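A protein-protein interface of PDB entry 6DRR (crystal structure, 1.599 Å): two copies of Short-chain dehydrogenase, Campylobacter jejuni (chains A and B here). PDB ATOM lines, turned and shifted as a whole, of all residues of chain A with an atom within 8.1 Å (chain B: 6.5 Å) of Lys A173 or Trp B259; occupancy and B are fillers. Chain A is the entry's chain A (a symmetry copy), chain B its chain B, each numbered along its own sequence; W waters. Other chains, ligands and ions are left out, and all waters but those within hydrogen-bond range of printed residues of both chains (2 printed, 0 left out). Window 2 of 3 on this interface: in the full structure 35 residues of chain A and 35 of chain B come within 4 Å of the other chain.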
ATOM      1  N   LYS A 129      25.648   5.106  -4.510  1.00  0.00           N
ATOM      2  CA  LYS A 129      26.104   4.271  -5.618  1.00  0.00           C
ATOM      3  C   LYS A 129      27.100   3.224  -5.133  1.00  0.00           C
ATOM      4  O   LYS A 129      27.018   2.054  -5.518  1.00  0.00           O
ATOM      5  CB  LYS A 129      26.716   5.140  -6.717  1.00  0.00           C
ATOM      6  CG  LYS A 129      25.690   5.928  -7.530  1.00  0.00           C
ATOM      7  CD  LYS A 129      26.375   7.037  -8.339  1.00  0.00           C
ATOM      8  CE  LYS A 129      27.113   6.485  -9.545  1.00  0.00           C
ATOM      9  NZ  LYS A 129      27.995   7.506 -10.226  1.00  0.00           N
ATOM     10  N   GLN A 132      25.249   0.454  -3.589  1.00  0.00           N
ATOM     11  CA  GLN A 132      24.127   0.004  -4.419  1.00  0.00           C
ATOM     12  C   GLN A 132      22.808   0.086  -3.651  1.00  0.00           C
ATOM     13  O   GLN A 132      22.072  -0.895  -3.502  1.00  0.00           O
ATOM     14  CB  GLN A 132      24.370  -1.405  -4.962  1.00  0.00           C
ATOM     15  CG  GLN A 132      25.619  -1.485  -5.805  1.00  0.00           C
ATOM     16  CD  GLN A 132      25.943  -2.892  -6.267  1.00  0.00           C
ATOM     17  OE1 GLN A 132      25.053  -3.710  -6.511  1.00  0.00           O
ATOM     18  NE2 GLN A 132      27.236  -3.185  -6.379  1.00  0.00           N
ATOM     19  N   TRP A 167      15.925   9.755 -12.130  1.00  0.00           N
ATOM     20  CA  TRP A 167      17.034   9.149 -11.393  1.00  0.00           C
ATOM     21  C   TRP A 167      16.972   7.635 -11.463  1.00  0.00           C
ATOM     22  O   TRP A 167      18.018   6.974 -11.459  1.00  0.00           O
ATOM     23  CB  TRP A 167      17.033   9.613  -9.933  1.00  0.00           C
ATOM     24  CG  TRP A 167      17.212  11.109  -9.775  1.00  0.00           C
ATOM     25  CD1 TRP A 167      17.786  11.975 -10.679  1.00  0.00           C
ATOM     26  CD2 TRP A 167      16.809  11.907  -8.655  1.00  0.00           C
ATOM     27  NE1 TRP A 167      17.745  13.258 -10.186  1.00  0.00           N
ATOM     28  CE2 TRP A 167      17.158  13.245  -8.946  1.00  0.00           C
ATOM     29  CE3 TRP A 167      16.172  11.624  -7.438  1.00  0.00           C
ATOM     30  CZ2 TRP A 167      16.898  14.297  -8.058  1.00  0.00           C
ATOM     31  CZ3 TRP A 167      15.918  12.666  -6.554  1.00  0.00           C
ATOM     32  CH2 TRP A 167      16.287  13.986  -6.869  1.00  0.00           C
ATOM     33  N   ALA A 168      15.770   7.062 -11.554  1.00  0.00           N
ATOM     34  CA  ALA A 168      15.685   5.622 -11.774  1.00  0.00           C
ATOM     35  C   ALA A 168      16.363   5.228 -13.082  1.00  0.00           C
ATOM     36  O   ALA A 168      17.126   4.254 -13.119  1.00  0.00           O
ATOM     37  CB  ALA A 168      14.223   5.163 -11.753  1.00  0.00           C
ATOM     38  N   CYS A 169      16.114   5.988 -14.157  1.00  0.00           N
ATOM     39  CA  CYS A 169      16.836   5.789 -15.412  1.00  0.00           C
ATOM     40  C   CYS A 169      18.336   5.986 -15.233  1.00  0.00           C
ATOM     41  O   CYS A 169      19.142   5.200 -15.745  1.00  0.00           O
ATOM     42  CB  CYS A 169      16.337   6.768 -16.472  1.00  0.00           C
ATOM     43  SG  CYS A 169      14.700   6.426 -17.156  1.00  0.00           S
ATOM     44  N   ALA A 170      18.726   7.079 -14.563  1.00  0.00           N
ATOM     45  CA  ALA A 170      20.137   7.463 -14.499  1.00  0.00           C
ATOM     46  C   ALA A 170      20.981   6.408 -13.808  1.00  0.00           C
ATOM     47  O   ALA A 170      22.129   6.169 -14.198  1.00  0.00           O
ATOM     48  CB  ALA A 170      20.278   8.800 -13.766  1.00  0.00           C
ATOM     49  N   PHE A 171      20.440   5.764 -12.780  1.00  0.00           N
ATOM     50  CA  PHE A 171      21.264   4.958 -11.888  1.00  0.00           C
ATOM     51  C   PHE A 171      20.884   3.484 -11.863  1.00  0.00           C
ATOM     52  O   PHE A 171      21.463   2.722 -11.077  1.00  0.00           O
ATOM     53  CB  PHE A 171      21.227   5.586 -10.491  1.00  0.00           C
ATOM     54  CG  PHE A 171      21.592   7.041 -10.522  1.00  0.00           C
ATOM     55  CD1 PHE A 171      22.836   7.424 -11.012  1.00  0.00           C
ATOM     56  CD2 PHE A 171      20.685   8.020 -10.142  1.00  0.00           C
ATOM     57  CE1 PHE A 171      23.184   8.760 -11.095  1.00  0.00           C
ATOM     58  CE2 PHE A 171      21.025   9.359 -10.218  1.00  0.00           C
ATOM     59  CZ  PHE A 171      22.279   9.725 -10.697  1.00  0.00           C
ATOM     60  N   ALA A 172      19.964   3.048 -12.733  1.00  0.00           N
ATOM     61  CA  ALA A 172      19.672   1.619 -12.827  1.00  0.00           C
ATOM     62  C   ALA A 172      20.932   0.836 -13.167  1.00  0.00           C
ATOM     63  O   ALA A 172      21.165  -0.249 -12.622  1.00  0.00           O
ATOM     64  CB  ALA A 172      18.581   1.371 -13.874  1.00  0.00           C
ATOM     65  N   LYS A 173      21.774   1.391 -14.044  1.00  0.00           N
ATOM     66  CA  LYS A 173      23.045   0.747 -14.379  1.00  0.00           C
ATOM     67  C   LYS A 173      23.918   0.551 -13.146  1.00  0.00           C
ATOM     68  O   LYS A 173      24.687  -0.412 -13.076  1.00  0.00           O
ATOM     69  CB  LYS A 173      23.791   1.572 -15.431  1.00  0.00           C
ATOM     70  N   ASP A 174      23.792   1.427 -12.155  1.00  0.00           N
ATOM     71  CA  ASP A 174      24.579   1.366 -10.936  1.00  0.00           C
ATOM     72  C   ASP A 174      23.943   0.497  -9.865  1.00  0.00           C
ATOM     73  O   ASP A 174      24.471   0.424  -8.747  1.00  0.00           O
ATOM     74  CB  ASP A 174      24.779   2.787 -10.396  1.00  0.00           C
ATOM     75  CG  ASP A 174      25.403   3.709 -11.423  1.00  0.00           C
ATOM     76  OD1 ASP A 174      26.555   3.447 -11.823  1.00  0.00           O
ATOM     77  OD2 ASP A 174      24.740   4.677 -11.855  1.00  0.00           O
ATOM     78  N   ASN A 175      22.803  -0.132 -10.167  1.00  0.00           N
ATOM     79  CA  ASN A 175      22.016  -0.883  -9.187  1.00  0.00           C
ATOM     80  C   ASN A 175      21.611  -0.010  -8.004  1.00  0.00           C
ATOM     81  O   ASN A 175      21.614  -0.448  -6.845  1.00  0.00           O
ATOM     82  CB  ASN A 175      22.741  -2.137  -8.698  1.00  0.00           C
ATOM     83  CG  ASN A 175      21.807  -3.085  -7.987  1.00  0.00           C
ATOM     84  OD1 ASN A 175      20.605  -3.107  -8.275  1.00  0.00           O
ATOM     85  ND2 ASN A 175      22.336  -3.852  -7.041  1.00  0.00           N
ATOM     86  N   VAL A 176      21.238   1.234  -8.294  1.00  0.00           N
ATOM     87  CA  VAL A 176      20.608   2.115  -7.321  1.00  0.00           C
ATOM     88  C   VAL A 176      19.127   2.212  -7.670  1.00  0.00           C
ATOM     89  O   VAL A 176      18.772   2.555  -8.800  1.00  0.00           O
ATOM     90  CB  VAL A 176      21.267   3.502  -7.311  1.00  0.00           C
ATOM     91  CG1 VAL A 176      20.453   4.468  -6.479  1.00  0.00           C
ATOM     92  CG2 VAL A 176      22.680   3.382  -6.756  1.00  0.00           C
ATOM     93  N   ILE B 212      15.780  -4.770 -19.709  1.00  0.00           N
ATOM     94  CA  ILE B 212      15.379  -4.583 -18.316  1.00  0.00           C
ATOM     95  C   ILE B 212      16.363  -3.607 -17.669  1.00  0.00           C
ATOM     96  O   ILE B 212      17.520  -3.984 -17.416  1.00  0.00           O
ATOM     97  CB  ILE B 212      15.331  -5.912 -17.558  1.00  0.00           C
ATOM     98  CG1 ILE B 212      14.444  -6.910 -18.310  1.00  0.00           C
ATOM     99  CG2 ILE B 212      14.826  -5.684 -16.119  1.00  0.00           C
ATOM    100  CD1 ILE B 212      14.499  -8.308 -17.730  1.00  0.00           C
ATOM    101  N   PRO B 213      15.943  -2.379 -17.350  1.00  0.00           N
ATOM    102  CA  PRO B 213      16.903  -1.363 -16.887  1.00  0.00           C
ATOM    103  C   PRO B 213      17.696  -1.761 -15.653  1.00  0.00           C
ATOM    104  O   PRO B 213      18.911  -1.513 -15.593  1.00  0.00           O
ATOM    105  CB  PRO B 213      15.993  -0.153 -16.617  1.00  0.00           C
ATOM    106  CG  PRO B 213      14.853  -0.340 -17.563  1.00  0.00           C
ATOM    107  CD  PRO B 213      14.617  -1.812 -17.643  1.00  0.00           C
ATOM    108  N   LEU B 214      17.058  -2.372 -14.659  1.00  0.00           N
ATOM    109  CA  LEU B 214      17.738  -2.631 -13.393  1.00  0.00           C
ATOM    110  C   LEU B 214      18.523  -3.935 -13.520  1.00  0.00           C
ATOM    111  O   LEU B 214      18.013  -5.033 -13.292  1.00  0.00           O
ATOM    112  CB  LEU B 214      16.732  -2.659 -12.254  1.00  0.00           C
ATOM    113  CG  LEU B 214      17.315  -2.546 -10.848  1.00  0.00           C
ATOM    114  CD1 LEU B 214      18.248  -1.323 -10.686  1.00  0.00           C
ATOM    115  CD2 LEU B 214      16.158  -2.500  -9.867  1.00  0.00           C
ATOM    116  N   GLY B 215      19.789  -3.809 -13.922  1.00  0.00           N
ATOM    117  CA  GLY B 215      20.706  -4.930 -13.948  1.00  0.00           C
ATOM    118  C   GLY B 215      20.746  -5.752 -15.222  1.00  0.00           C
ATOM    119  O   GLY B 215      21.536  -6.709 -15.290  1.00  0.00           O
ATOM    120  N   HIS B 216      19.935  -5.425 -16.232  1.00  0.00           N
ATOM    121  CA  HIS B 216      19.829  -6.243 -17.445  1.00  0.00           C
ATOM    122  C   HIS B 216      19.670  -7.722 -17.098  1.00  0.00           C
ATOM    123  O   HIS B 216      20.375  -8.588 -17.620  1.00  0.00           O
ATOM    124  CB  HIS B 216      21.041  -6.050 -18.356  1.00  0.00           C
ATOM    125  CG  HIS B 216      21.083  -4.728 -19.055  1.00  0.00           C
ATOM    126  ND1 HIS B 216      22.069  -4.410 -19.965  1.00  0.00           N
ATOM    127  CD2 HIS B 216      20.267  -3.648 -18.991  1.00  0.00           C
ATOM    128  CE1 HIS B 216      21.862  -3.192 -20.432  1.00  0.00           C
ATOM    129  NE2 HIS B 216      20.778  -2.704 -19.852  1.00  0.00           N
ATOM    130  N   ARG B 217      18.748  -8.012 -16.183  1.00  0.00           N
ATOM    131  CA  ARG B 217      18.557  -9.375 -15.711  1.00  0.00           C
ATOM    132  C   ARG B 217      17.099  -9.542 -15.322  1.00  0.00           C
ATOM    133  O   ARG B 217      16.413  -8.568 -15.013  1.00  0.00           O
ATOM    134  CB  ARG B 217      19.497  -9.698 -14.538  1.00  0.00           C
ATOM    135  CG  ARG B 217      19.455  -8.710 -13.380  1.00  0.00           C
ATOM    136  CD  ARG B 217      18.602  -9.243 -12.252  1.00  0.00           C
ATOM    137  NE  ARG B 217      18.597  -8.401 -11.055  1.00  0.00           N
ATOM    138  CZ  ARG B 217      17.651  -8.490 -10.127  1.00  0.00           C
ATOM    139  NH1 ARG B 217      16.664  -9.364 -10.290  1.00  0.00           N
ATOM    140  NH2 ARG B 217      17.668  -7.705  -9.060  1.00  0.00           N
ATOM    141  N   LEU B 257      16.342   3.440 -22.939  1.00  0.00           N
ATOM    142  CA  LEU B 257      17.428   3.370 -21.970  1.00  0.00           C
ATOM    143  C   LEU B 257      18.391   2.246 -22.334  1.00  0.00           C
ATOM    144  O   LEU B 257      17.972   1.131 -22.665  1.00  0.00           O
ATOM    145  CB  LEU B 257      16.855   3.156 -20.566  1.00  0.00           C
ATOM    146  CG  LEU B 257      17.783   3.342 -19.374  1.00  0.00           C
ATOM    147  CD1 LEU B 257      18.327   4.747 -19.342  1.00  0.00           C
ATOM    148  CD2 LEU B 257      17.007   3.034 -18.097  1.00  0.00           C
ATOM    149  N   ASN B 258      19.687   2.553 -22.299  1.00  0.00           N
ATOM    150  CA  ASN B 258      20.714   1.538 -22.489  1.00  0.00           C
ATOM    151  C   ASN B 258      21.930   1.922 -21.655  1.00  0.00           C
ATOM    152  O   ASN B 258      21.954   2.966 -20.998  1.00  0.00           O
ATOM    153  CB  ASN B 258      21.045   1.357 -23.976  1.00  0.00           C
ATOM    154  CG  ASN B 258      21.548   2.626 -24.623  1.00  0.00           C
ATOM    155  OD1 ASN B 258      22.464   3.269 -24.121  1.00  0.00           O
ATOM    156  ND2 ASN B 258      20.952   2.990 -25.751  1.00  0.00           N
ATOM    157  N   TRP B 259      22.946   1.065 -21.678  1.00  0.00           N
ATOM    158  CA  TRP B 259      24.114   1.275 -20.835  1.00  0.00           C
ATOM    159  C   TRP B 259      25.208   2.086 -21.520  1.00  0.00           C
ATOM    160  O   TRP B 259      26.262   2.309 -20.915  1.00  0.00           O
ATOM    161  CB  TRP B 259      24.658  -0.073 -20.363  1.00  0.00           C
ATOM    162  CG  TRP B 259      23.854  -0.622 -19.225  1.00  0.00           C
ATOM    163  CD1 TRP B 259      22.803  -0.012 -18.604  1.00  0.00           C
ATOM    164  CD2 TRP B 259      24.045  -1.875 -18.556  1.00  0.00           C
ATOM    165  NE1 TRP B 259      22.318  -0.812 -17.595  1.00  0.00           N
ATOM    166  CE2 TRP B 259      23.064  -1.961 -17.544  1.00  0.00           C
ATOM    167  CE3 TRP B 259      24.942  -2.940 -18.724  1.00  0.00           C
ATOM    168  CZ2 TRP B 259      22.956  -3.069 -16.697  1.00  0.00           C
ATOM    169  CZ3 TRP B 259      24.835  -4.039 -17.884  1.00  0.00           C
ATOM    170  CH2 TRP B 259      23.850  -4.093 -16.882  1.00  0.00           C
ATOM    171  N   ASP B 260      24.981   2.540 -22.750  1.00  0.00           N
ATOM    172  CA  ASP B 260      25.935   3.410 -23.433  1.00  0.00           C
ATOM    173  C   ASP B 260      26.022   4.770 -22.746  1.00  0.00           C
ATOM    174  O   ASP B 260      27.037   5.460 -22.844  1.00  0.00           O
ATOM    175  CB  ASP B 260      25.546   3.589 -24.901  1.00  0.00           C
ATOM    176  CG  ASP B 260      25.322   2.268 -25.607  1.00  0.00           C
ATOM    177  OD1 ASP B 260      25.491   1.210 -24.965  1.00  0.00           O
ATOM    178  OD2 ASP B 260      24.970   2.290 -26.804  1.00  0.00           O
HETATM  179  O   HOH W   1      20.541  -4.046 -10.841  1.00  0.00           O
HETATM  180  O   HOH W   2      22.382  -2.747 -12.540  1.00  0.00           O
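The side-chain amide nitrogen of Asn A175 is in hydrogen-bond range of the side-chain amide oxygen of Gln A132 (2.8 Å). NE1 of Trp B259 sits at hydrogen-bond distance from NE2 of His B216 (3.3 Å).
CD1 of Leu B257 touches O of Cys A169, 3.7 Å away. Ala A172 touches Pro B213 (CB to O, 3.4 Å). Leu B214 touches Ala A172 (CD1 to O, 3.7 Å). CB of Lys A173 touches NE1 of Trp B259, at 3.5 Å. Asn A175 touches Leu B214 (OD1 to CD1, 3.8 Å).
Printed residues of chain B within 4 Å of Lys A173: Trp B259 (3.5 Å). Of chain A, only Lys A173 (3.5 Å) comes within 4 Å of Trp B259. Of the printed residues of chain A, Leu B257 touches Cys A169. Of the printed residues of chain A, Leu B214 touches Ala A172 and Asn A175. Printed residues of chain A within 4 Å of Pro B213: Ala A172 (3.4 Å). His B216 touches none of the printed residues of chain A. Ala A168 touches none of the printed residues of chain B. The nearest residue of chain A that does not touch Trp B259 is Ala A172 (4.9 Å). The nearest printed residue of chain B that does not touch Asn A175 is Arg B217 (5.5 Å).
Printed residues of chain A that touch a printed residue of chain B: Cys A169, Ala A172, Lys A173 and Asn A175. Hydrophobic or aromatic side chains of chain A within 4 Å of the printed part of chain B: Ala A172. Along chain A the printed residues that touch a printed residue of chain B span positions 169 to 175. Hydrophobic or aromatic side chains of chain B that line the printed part of chain A: Leu B214, Leu B257 and Trp B259. Among the printed residues, 5 pairs touch across the chains. Among the printed residues, no Asp or Glu carboxylate lies within 4 Å of a Lys or Arg side-chain nitrogen of the other chain.
No position is printed for both chains. Of the 5 pairs that touch across the chains among the printed residues, none has its exchanged pair printed and touching as well.
Water W1 lies within hydrogen-bond range of the side-chain amide oxygen (OD1) of Asn A175 (2.7 Å) and the backbone NH (N) of Gly B215 (3.2 Å). Water W2 lies within hydrogen-bond range of the backbone carbonyl oxygen of Ala A172 (2.8 Å), the backbone NH of Gly B215 (3.1 Å) and the backbone carbonyl oxygen of Lys A173 (3.3 Å).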
